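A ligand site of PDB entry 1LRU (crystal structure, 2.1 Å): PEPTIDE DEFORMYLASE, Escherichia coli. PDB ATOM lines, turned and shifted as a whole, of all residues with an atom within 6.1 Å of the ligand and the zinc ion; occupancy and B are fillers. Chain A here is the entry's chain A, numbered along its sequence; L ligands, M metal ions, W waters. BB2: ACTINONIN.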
ATOM      1  N   GLU A  41      26.270   7.010  24.137  1.00  0.00           N
ATOM      2  CA  GLU A  41      26.311   7.537  22.776  1.00  0.00           C
ATOM      3  C   GLU A  41      24.931   7.782  22.184  1.00  0.00           C
ATOM      4  O   GLU A  41      24.811   8.091  21.008  1.00  0.00           O
ATOM      5  CB  GLU A  41      27.105   6.607  21.858  1.00  0.00           C
ATOM      6  CG  GLU A  41      28.488   6.238  22.386  1.00  0.00           C
ATOM      7  CD  GLU A  41      29.359   7.449  22.644  1.00  0.00           C
ATOM      8  OE1 GLU A  41      29.540   8.261  21.716  1.00  0.00           O
ATOM      9  OE2 GLU A  41      29.861   7.591  23.786  1.00  0.00           O
ATOM     10  N   GLU A  42      23.906   7.660  23.017  1.00  0.00           N
ATOM     11  CA  GLU A  42      22.540   7.890  22.576  1.00  0.00           C
ATOM     12  C   GLU A  42      22.111   6.941  21.442  1.00  0.00           C
ATOM     13  O   GLU A  42      21.390   7.333  20.521  1.00  0.00           O
ATOM     14  CB  GLU A  42      22.345   9.368  22.182  1.00  0.00           C
ATOM     15  CG  GLU A  42      22.555  10.362  23.333  1.00  0.00           C
ATOM     16  CD  GLU A  42      22.522  11.821  22.886  1.00  0.00           C
ATOM     17  OE1 GLU A  42      21.580  12.222  22.177  1.00  0.00           O
ATOM     18  OE2 GLU A  42      23.449  12.585  23.265  1.00  0.00           O
ATOM     19  N   GLY A  43      22.579   5.705  21.519  1.00  0.00           N
ATOM     20  CA  GLY A  43      22.224   4.702  20.537  1.00  0.00           C
ATOM     21  C   GLY A  43      21.100   3.848  21.099  1.00  0.00           C
ATOM     22  O   GLY A  43      20.929   3.733  22.301  1.00  0.00           O
ATOM     23  N   ILE A  44      20.305   3.266  20.207  1.00  0.00           N
ATOM     24  CA  ILE A  44      19.200   2.414  20.618  1.00  0.00           C
ATOM     25  C   ILE A  44      19.618   0.918  20.602  1.00  0.00           C
ATOM     26  O   ILE A  44      18.928   0.046  21.175  1.00  0.00           O
ATOM     27  CB  ILE A  44      17.930   2.775  19.759  1.00  0.00           C
ATOM     28  CG1 ILE A  44      16.914   3.484  20.640  1.00  0.00           C
ATOM     29  CG2 ILE A  44      17.313   1.574  19.084  1.00  0.00           C
ATOM     30  CD1 ILE A  44      17.424   4.784  21.218  1.00  0.00           C
ATOM     31  N   GLY A  45      20.776   0.640  20.015  1.00  0.00           N
ATOM     32  CA  GLY A  45      21.268  -0.719  19.955  1.00  0.00           C
ATOM     33  C   GLY A  45      22.778  -0.722  19.846  1.00  0.00           C
ATOM     34  O   GLY A  45      23.366   0.340  19.554  1.00  0.00           O
ATOM     35  N   LEU A  46      23.406  -1.885  20.078  1.00  0.00           N
ATOM     36  CA  LEU A  46      24.860  -2.029  19.991  1.00  0.00           C
ATOM     37  C   LEU A  46      25.298  -3.507  19.810  1.00  0.00           C
ATOM     38  O   LEU A  46      24.675  -4.416  20.350  1.00  0.00           O
ATOM     39  CB  LEU A  46      25.538  -1.433  21.233  1.00  0.00           C
ATOM     40  CG  LEU A  46      27.021  -1.096  21.107  1.00  0.00           C
ATOM     41  CD1 LEU A  46      27.206   0.194  20.323  1.00  0.00           C
ATOM     42  CD2 LEU A  46      27.610  -0.953  22.477  1.00  0.00           C
ATOM     43  N   ALA A  47      26.313  -3.709  18.977  1.00  0.00           N
ATOM     44  CA  ALA A  47      26.883  -5.029  18.703  1.00  0.00           C
ATOM     45  C   ALA A  47      28.354  -5.006  19.177  1.00  0.00           C
ATOM     46  O   ALA A  47      29.067  -4.014  18.953  1.00  0.00           O
ATOM     47  CB  ALA A  47      26.800  -5.349  17.225  1.00  0.00           C
ATOM     48  N   GLN A  50      31.614  -3.355  17.308  1.00  0.00           N
ATOM     49  CA  GLN A  50      31.875  -1.903  17.258  1.00  0.00           C
ATOM     50  C   GLN A  50      32.795  -1.461  18.356  1.00  0.00           C
ATOM     51  O   GLN A  50      33.402  -0.393  18.292  1.00  0.00           O
ATOM     52  CB  GLN A  50      30.572  -1.146  17.413  1.00  0.00           C
ATOM     53  CG  GLN A  50      29.484  -1.563  16.475  1.00  0.00           C
ATOM     54  CD  GLN A  50      28.259  -0.701  16.644  1.00  0.00           C
ATOM     55  OE1 GLN A  50      27.218  -1.184  17.075  1.00  0.00           O
ATOM     56  NE2 GLN A  50      28.382   0.578  16.308  1.00  0.00           N
ATOM     57  N   ILE A  86      13.826   2.814   7.037  1.00  0.00           N
ATOM     58  CA  ILE A  86      13.787   4.113   7.697  1.00  0.00           C
ATOM     59  C   ILE A  86      15.182   4.681   7.515  1.00  0.00           C
ATOM     60  O   ILE A  86      16.060   4.008   6.940  1.00  0.00           O
ATOM     61  CB  ILE A  86      13.428   4.021   9.210  1.00  0.00           C
ATOM     62  CG1 ILE A  86      14.459   3.139   9.958  1.00  0.00           C
ATOM     63  CG2 ILE A  86      11.965   3.518   9.381  1.00  0.00           C
ATOM     64  CD1 ILE A  86      14.177   3.019  11.456  1.00  0.00           C
ATOM     65  N   GLU A  87      15.379   5.942   7.904  1.00  0.00           N
ATOM     66  CA  GLU A  87      16.698   6.556   7.783  1.00  0.00           C
ATOM     67  C   GLU A  87      17.450   6.094   9.017  1.00  0.00           C
ATOM     68  O   GLU A  87      16.984   6.326  10.127  1.00  0.00           O
ATOM     69  CB  GLU A  87      16.622   8.096   7.718  1.00  0.00           C
ATOM     70  CG  GLU A  87      16.013   8.648   6.411  1.00  0.00           C
ATOM     71  CD  GLU A  87      16.183  10.169   6.205  1.00  0.00           C
ATOM     72  OE1 GLU A  87      17.001  10.822   6.863  1.00  0.00           O
ATOM     73  OE2 GLU A  87      15.480  10.708   5.334  1.00  0.00           O
ATOM     74  N   GLU A  88      18.537   5.367   8.809  1.00  0.00           N
ATOM     75  CA  GLU A  88      19.324   4.807   9.909  1.00  0.00           C
ATOM     76  C   GLU A  88      20.636   5.504  10.032  1.00  0.00           C
ATOM     77  O   GLU A  88      21.236   5.923   9.045  1.00  0.00           O
ATOM     78  CB  GLU A  88      19.645   3.329   9.667  1.00  0.00           C
ATOM     79  CG  GLU A  88      18.461   2.416   9.464  1.00  0.00           C
ATOM     80  CD  GLU A  88      18.857   0.970   9.221  1.00  0.00           C
ATOM     81  OE1 GLU A  88      19.981   0.561   9.577  1.00  0.00           O
ATOM     82  OE2 GLU A  88      18.032   0.215   8.678  1.00  0.00           O
ATOM     83  N   GLY A  89      21.081   5.650  11.258  1.00  0.00           N
ATOM     84  CA  GLY A  89      22.373   6.242  11.498  1.00  0.00           C
ATOM     85  C   GLY A  89      23.121   5.143  12.237  1.00  0.00           C
ATOM     86  O   GLY A  89      22.497   4.231  12.802  1.00  0.00           O
ATOM     87  N   CYS A  90      24.434   5.233  12.254  1.00  0.00           N
ATOM     88  CA  CYS A  90      25.233   4.227  12.939  1.00  0.00           C
ATOM     89  C   CYS A  90      26.325   4.925  13.742  1.00  0.00           C
ATOM     90  O   CYS A  90      26.913   5.908  13.275  1.00  0.00           O
ATOM     91  CB  CYS A  90      25.848   3.257  11.906  1.00  0.00           C
ATOM     92  SG  CYS A  90      27.136   2.088  12.556  1.00  0.00           S
ATOM     93  N   LEU A  91      26.574   4.461  14.967  1.00  0.00           N
ATOM     94  CA  LEU A  91      27.614   5.060  15.811  1.00  0.00           C
ATOM     95  C   LEU A  91      28.990   4.921  15.135  1.00  0.00           C
ATOM     96  O   LEU A  91      29.847   5.802  15.264  1.00  0.00           O
ATOM     97  CB  LEU A  91      27.604   4.425  17.213  1.00  0.00           C
ATOM     98  CG  LEU A  91      26.340   4.583  18.083  1.00  0.00           C
ATOM     99  CD1 LEU A  91      26.395   3.704  19.325  1.00  0.00           C
ATOM    100  CD2 LEU A  91      26.160   6.039  18.509  1.00  0.00           C
ATOM    101  N   SER A  92      29.180   3.869  14.342  1.00  0.00           N
ATOM    102  CA  SER A  92      30.446   3.654  13.636  1.00  0.00           C
ATOM    103  C   SER A  92      30.611   4.538  12.393  1.00  0.00           C
ATOM    104  O   SER A  92      31.710   4.669  11.841  1.00  0.00           O
ATOM    105  CB  SER A  92      30.592   2.163  13.291  1.00  0.00           C
ATOM    106  OG  SER A  92      30.551   1.367  14.471  1.00  0.00           O
ATOM    107  N   ARG A  97      23.159   9.590   8.115  1.00  0.00           N
ATOM    108  CA  ARG A  97      21.901   8.832   8.081  1.00  0.00           C
ATOM    109  C   ARG A  97      21.489   8.533   6.668  1.00  0.00           C
ATOM    110  O   ARG A  97      21.711   9.357   5.769  1.00  0.00           O
ATOM    111  CB  ARG A  97      20.770   9.582   8.781  1.00  0.00           C
ATOM    112  CG  ARG A  97      21.012   9.782  10.235  1.00  0.00           C
ATOM    113  CD  ARG A  97      19.739   9.985  11.001  1.00  0.00           C
ATOM    114  NE  ARG A  97      20.054  10.287  12.379  1.00  0.00           N
ATOM    115  CZ  ARG A  97      19.225  10.855  13.248  1.00  0.00           C
ATOM    116  NH1 ARG A  97      17.994  11.199  12.888  1.00  0.00           N
ATOM    117  NH2 ARG A  97      19.645  11.141  14.479  1.00  0.00           N
ATOM    118  N   LEU A 125      10.425  -0.984  14.169  1.00  0.00           N
ATOM    119  CA  LEU A 125      11.777  -0.563  14.497  1.00  0.00           C
ATOM    120  C   LEU A 125      12.662  -1.656  15.123  1.00  0.00           C
ATOM    121  O   LEU A 125      13.889  -1.630  14.923  1.00  0.00           O
ATOM    122  CB  LEU A 125      11.749   0.658  15.406  1.00  0.00           C
ATOM    123  CG  LEU A 125      13.092   1.281  15.804  1.00  0.00           C
ATOM    124  CD1 LEU A 125      13.871   1.792  14.607  1.00  0.00           C
ATOM    125  CD2 LEU A 125      12.825   2.404  16.779  1.00  0.00           C
ATOM    126  N   ILE A 128      14.105  -3.903  12.338  1.00  0.00           N
ATOM    127  CA  ILE A 128      15.134  -3.175  11.604  1.00  0.00           C
ATOM    128  C   ILE A 128      16.424  -3.077  12.433  1.00  0.00           C
ATOM    129  O   ILE A 128      17.537  -3.162  11.917  1.00  0.00           O
ATOM    130  CB  ILE A 128      14.599  -1.739  11.265  1.00  0.00           C
ATOM    131  CG1 ILE A 128      13.623  -1.823  10.100  1.00  0.00           C
ATOM    132  CG2 ILE A 128      15.742  -0.779  10.989  1.00  0.00           C
ATOM    133  CD1 ILE A 128      12.792  -0.573   9.927  1.00  0.00           C
ATOM    134  N   CYS A 129      16.240  -2.838  13.727  1.00  0.00           N
ATOM    135  CA  CYS A 129      17.359  -2.723  14.666  1.00  0.00           C
ATOM    136  C   CYS A 129      18.111  -4.068  14.797  1.00  0.00           C
ATOM    137  O   CYS A 129      19.348  -4.106  14.654  1.00  0.00           O
ATOM    138  CB  CYS A 129      16.819  -2.261  16.021  1.00  0.00           C
ATOM    139  SG  CYS A 129      18.070  -2.195  17.281  1.00  0.00           S
ATOM    140  N   HIS A 132      20.146  -4.725  11.845  1.00  0.00           N
ATOM    141  CA  HIS A 132      21.300  -3.850  11.743  1.00  0.00           C
ATOM    142  C   HIS A 132      22.421  -4.281  12.705  1.00  0.00           C
ATOM    143  O   HIS A 132      23.607  -4.180  12.386  1.00  0.00           O
ATOM    144  CB  HIS A 132      20.786  -2.407  11.949  1.00  0.00           C
ATOM    145  CG  HIS A 132      21.834  -1.414  12.314  1.00  0.00           C
ATOM    146  ND1 HIS A 132      22.162  -0.346  11.513  1.00  0.00           N
ATOM    147  CD2 HIS A 132      22.601  -1.297  13.431  1.00  0.00           C
ATOM    148  CE1 HIS A 132      23.077   0.390  12.114  1.00  0.00           C
ATOM    149  NE2 HIS A 132      23.361  -0.164  13.280  1.00  0.00           N
ATOM    150  N   GLU A 133      22.046  -4.757  13.895  1.00  0.00           N
ATOM    151  CA  GLU A 133      23.050  -5.218  14.862  1.00  0.00           C
ATOM    152  C   GLU A 133      23.674  -6.559  14.381  1.00  0.00           C
ATOM    153  O   GLU A 133      24.902  -6.679  14.322  1.00  0.00           O
ATOM    154  CB  GLU A 133      22.446  -5.406  16.247  1.00  0.00           C
ATOM    155  CG  GLU A 133      21.717  -4.197  16.837  1.00  0.00           C
ATOM    156  CD  GLU A 133      22.557  -2.940  16.863  1.00  0.00           C
ATOM    157  OE1 GLU A 133      23.742  -2.959  16.464  1.00  0.00           O
ATOM    158  OE2 GLU A 133      22.007  -1.920  17.292  1.00  0.00           O
ATOM    159  N   HIS A 136      26.272  -6.319  12.017  1.00  0.00           N
ATOM    160  CA  HIS A 136      27.531  -5.939  12.623  1.00  0.00           C
ATOM    161  C   HIS A 136      28.422  -7.118  12.966  1.00  0.00           C
ATOM    162  O   HIS A 136      29.615  -7.092  12.678  1.00  0.00           O
ATOM    163  CB  HIS A 136      27.274  -5.069  13.851  1.00  0.00           C
ATOM    164  CG  HIS A 136      27.398  -3.607  13.584  1.00  0.00           C
ATOM    165  ND1 HIS A 136      28.552  -3.051  13.060  1.00  0.00           N
ATOM    166  CD2 HIS A 136      26.515  -2.591  13.703  1.00  0.00           C
ATOM    167  CE1 HIS A 136      28.375  -1.764  12.876  1.00  0.00           C
ATOM    168  NE2 HIS A 136      27.143  -1.457  13.252  1.00  0.00           N
ATOM    169  N   LEU A 141      28.056  -3.236   7.397  1.00  0.00           N
ATOM    170  CA  LEU A 141      27.565  -1.925   7.819  1.00  0.00           C
ATOM    171  C   LEU A 141      26.462  -1.479   6.855  1.00  0.00           C
ATOM    172  O   LEU A 141      26.468  -1.876   5.684  1.00  0.00           O
ATOM    173  CB  LEU A 141      28.744  -0.946   7.793  1.00  0.00           C
ATOM    174  CG  LEU A 141      30.047  -1.245   8.589  1.00  0.00           C
ATOM    175  CD1 LEU A 141      31.131  -0.237   8.223  1.00  0.00           C
ATOM    176  CD2 LEU A 141      29.826  -1.222  10.096  1.00  0.00           C
ATOM    177  N   PHE A 142      25.498  -0.669   7.329  1.00  0.00           N
ATOM    178  CA  PHE A 142      24.373  -0.191   6.495  1.00  0.00           C
ATOM    179  C   PHE A 142      24.727   0.487   5.152  1.00  0.00           C
ATOM    180  O   PHE A 142      24.018   0.335   4.135  1.00  0.00           O
ATOM    181  CB  PHE A 142      23.385   0.664   7.333  1.00  0.00           C
ATOM    182  CG  PHE A 142      23.798   2.113   7.535  1.00  0.00           C
ATOM    183  CD1 PHE A 142      23.719   3.025   6.483  1.00  0.00           C
ATOM    184  CD2 PHE A 142      24.215   2.567   8.773  1.00  0.00           C
ATOM    185  CE1 PHE A 142      24.057   4.391   6.670  1.00  0.00           C
ATOM    186  CE2 PHE A 142      24.552   3.916   8.974  1.00  0.00           C
ATOM    187  CZ  PHE A 142      24.473   4.828   7.922  1.00  0.00           C
HETATM  188  C5  BB2 L   1      23.252   2.484  17.100  1.00  0.00           C
HETATM  189  C3  BB2 L   1      24.172   1.496  16.398  1.00  0.00           C
HETATM  190  O4  BB2 L   1      25.168   1.877  15.738  1.00  0.00           O
HETATM  191  N1  BB2 L   1      23.945   0.212  16.456  1.00  0.00           N
HETATM  192  O2  BB2 L   1      24.792  -0.633  15.688  1.00  0.00           O
HETATM  193  C6  BB2 L   1      21.984   2.661  16.250  1.00  0.00           C
HETATM  194  C12 BB2 L   1      21.219   3.921  16.653  1.00  0.00           C
HETATM  195  O13 BB2 L   1      21.002   4.193  17.829  1.00  0.00           O
HETATM  196  C7  BB2 L   1      21.007   1.476  16.337  1.00  0.00           C
HETATM  197  C8  BB2 L   1      19.702   1.655  15.522  1.00  0.00           C
HETATM  198  C9  BB2 L   1      19.865   1.226  14.095  1.00  0.00           C
HETATM  199  C10 BB2 L   1      18.702   1.715  13.230  1.00  0.00           C
HETATM  200  C11 BB2 L   1      17.331   1.798  13.844  1.00  0.00           C
HETATM  201  N14 BB2 L   1      20.751   4.637  15.637  1.00  0.00           N
HETATM  202  C15 BB2 L   1      19.955   5.849  15.824  1.00  0.00           C
HETATM  203  C16 BB2 L   1      20.810   7.121  15.593  1.00  0.00           C
HETATM  204  C18 BB2 L   1      19.981   8.336  15.869  1.00  0.00           C
HETATM  205  C17 BB2 L   1      22.041   7.138  16.481  1.00  0.00           C
HETATM  206  C19 BB2 L   1      18.863   5.729  14.767  1.00  0.00           C
HETATM  207  O20 BB2 L   1      19.165   5.500  13.585  1.00  0.00           O
HETATM  208  N21 BB2 L   1      17.586   5.876  15.163  1.00  0.00           N
HETATM  209  C22 BB2 L   1      16.415   5.776  14.271  1.00  0.00           C
HETATM  210  C23 BB2 L   1      17.171   6.290  16.506  1.00  0.00           C
HETATM  211  C24 BB2 L   1      15.782   5.747  16.576  1.00  0.00           C
HETATM  212  C25 BB2 L   1      15.236   6.012  15.228  1.00  0.00           C
HETATM  213  C26 BB2 L   1      16.659   6.896  13.235  1.00  0.00           C
HETATM  214  O27 BB2 L   1      15.732   6.958  12.156  1.00  0.00           O
HETATM  215 ZN    ZN M   1      25.571   0.528  13.795  1.00  0.00          ZN
HETATM  216  O   HOH W   1      12.810   6.465  12.472  1.00  0.00           O
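O of Gly 89 sits at hydrogen-bond distance from N14 of the ligand, 3.4 Å away. The backbone NH (N) of Ile 44 is in hydrogen-bond range of an oxygen (O13) of the ligand (2.6 Å). The backbone carbonyl oxygen of Glu 87 sits at hydrogen-bond distance from an oxygen (O27) of the ligand. The backbone NH (N) of Leu 91 sits close to an oxygen (O4) of the ligand, at 3.0 Å. The side-chain carboxylate of Glu 133 sits at hydrogen-bond distance from a nitrogen (N1) of the ligand (3.0 Å). An oxygen (O20) of the ligand lies within hydrogen-bond range of the backbone NH (N) of Gly 89, at 3.0 Å. The backbone carbonyl oxygen (O) of Gly 45 is in hydrogen-bond range of a nitrogen (N1) of the ligand, 3.2 Å away. OE1 of Gln 50 lies close to O2 of the ligand (2.8 Å).
Gly 43 touches the ligand. Glu 88 touches the ligand (CA to O20, 3.7 Å). NH2 of Arg 97 touches C18 of the ligand, at 3.1 Å. CD1 of Leu 125 touches C11 of the ligand, 3.5 Å away. The nearest printed residue that does not touch the ligand is Glu 42 (4.1 Å).
Merely in contact with the zinc ion: Gln 50. The nearest printed residue that does not touch the zinc ion is Leu 91 (4.2 Å).
The side-chain carboxylate of Glu 133 lies within hydrogen-bond range of the backbone NH of Leu 46. OE1 of Glu 88 lies within hydrogen-bond range of ND1 of His 132 (3.1 Å). SG of Cys 90 lies close to N of Ser 92. N of Ala 47 sits at hydrogen-bond distance from OE1 of Gln 50 (3.3 Å). NE2 of Gln 50 is in hydrogen-bond range of OG of Ser 92.
An oxygen (O2) of the ligand binds the zinc ion, at 2.4 Å. A ring nitrogen (NE2) of His 132 is bound to the zinc ion (2.4 Å). An oxygen (O4) of the ligand is bound to the zinc ion. The zinc ion is bound by SG of Cys 90 (2.5 Å). The zinc ion is bound by NE2 of His 136.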
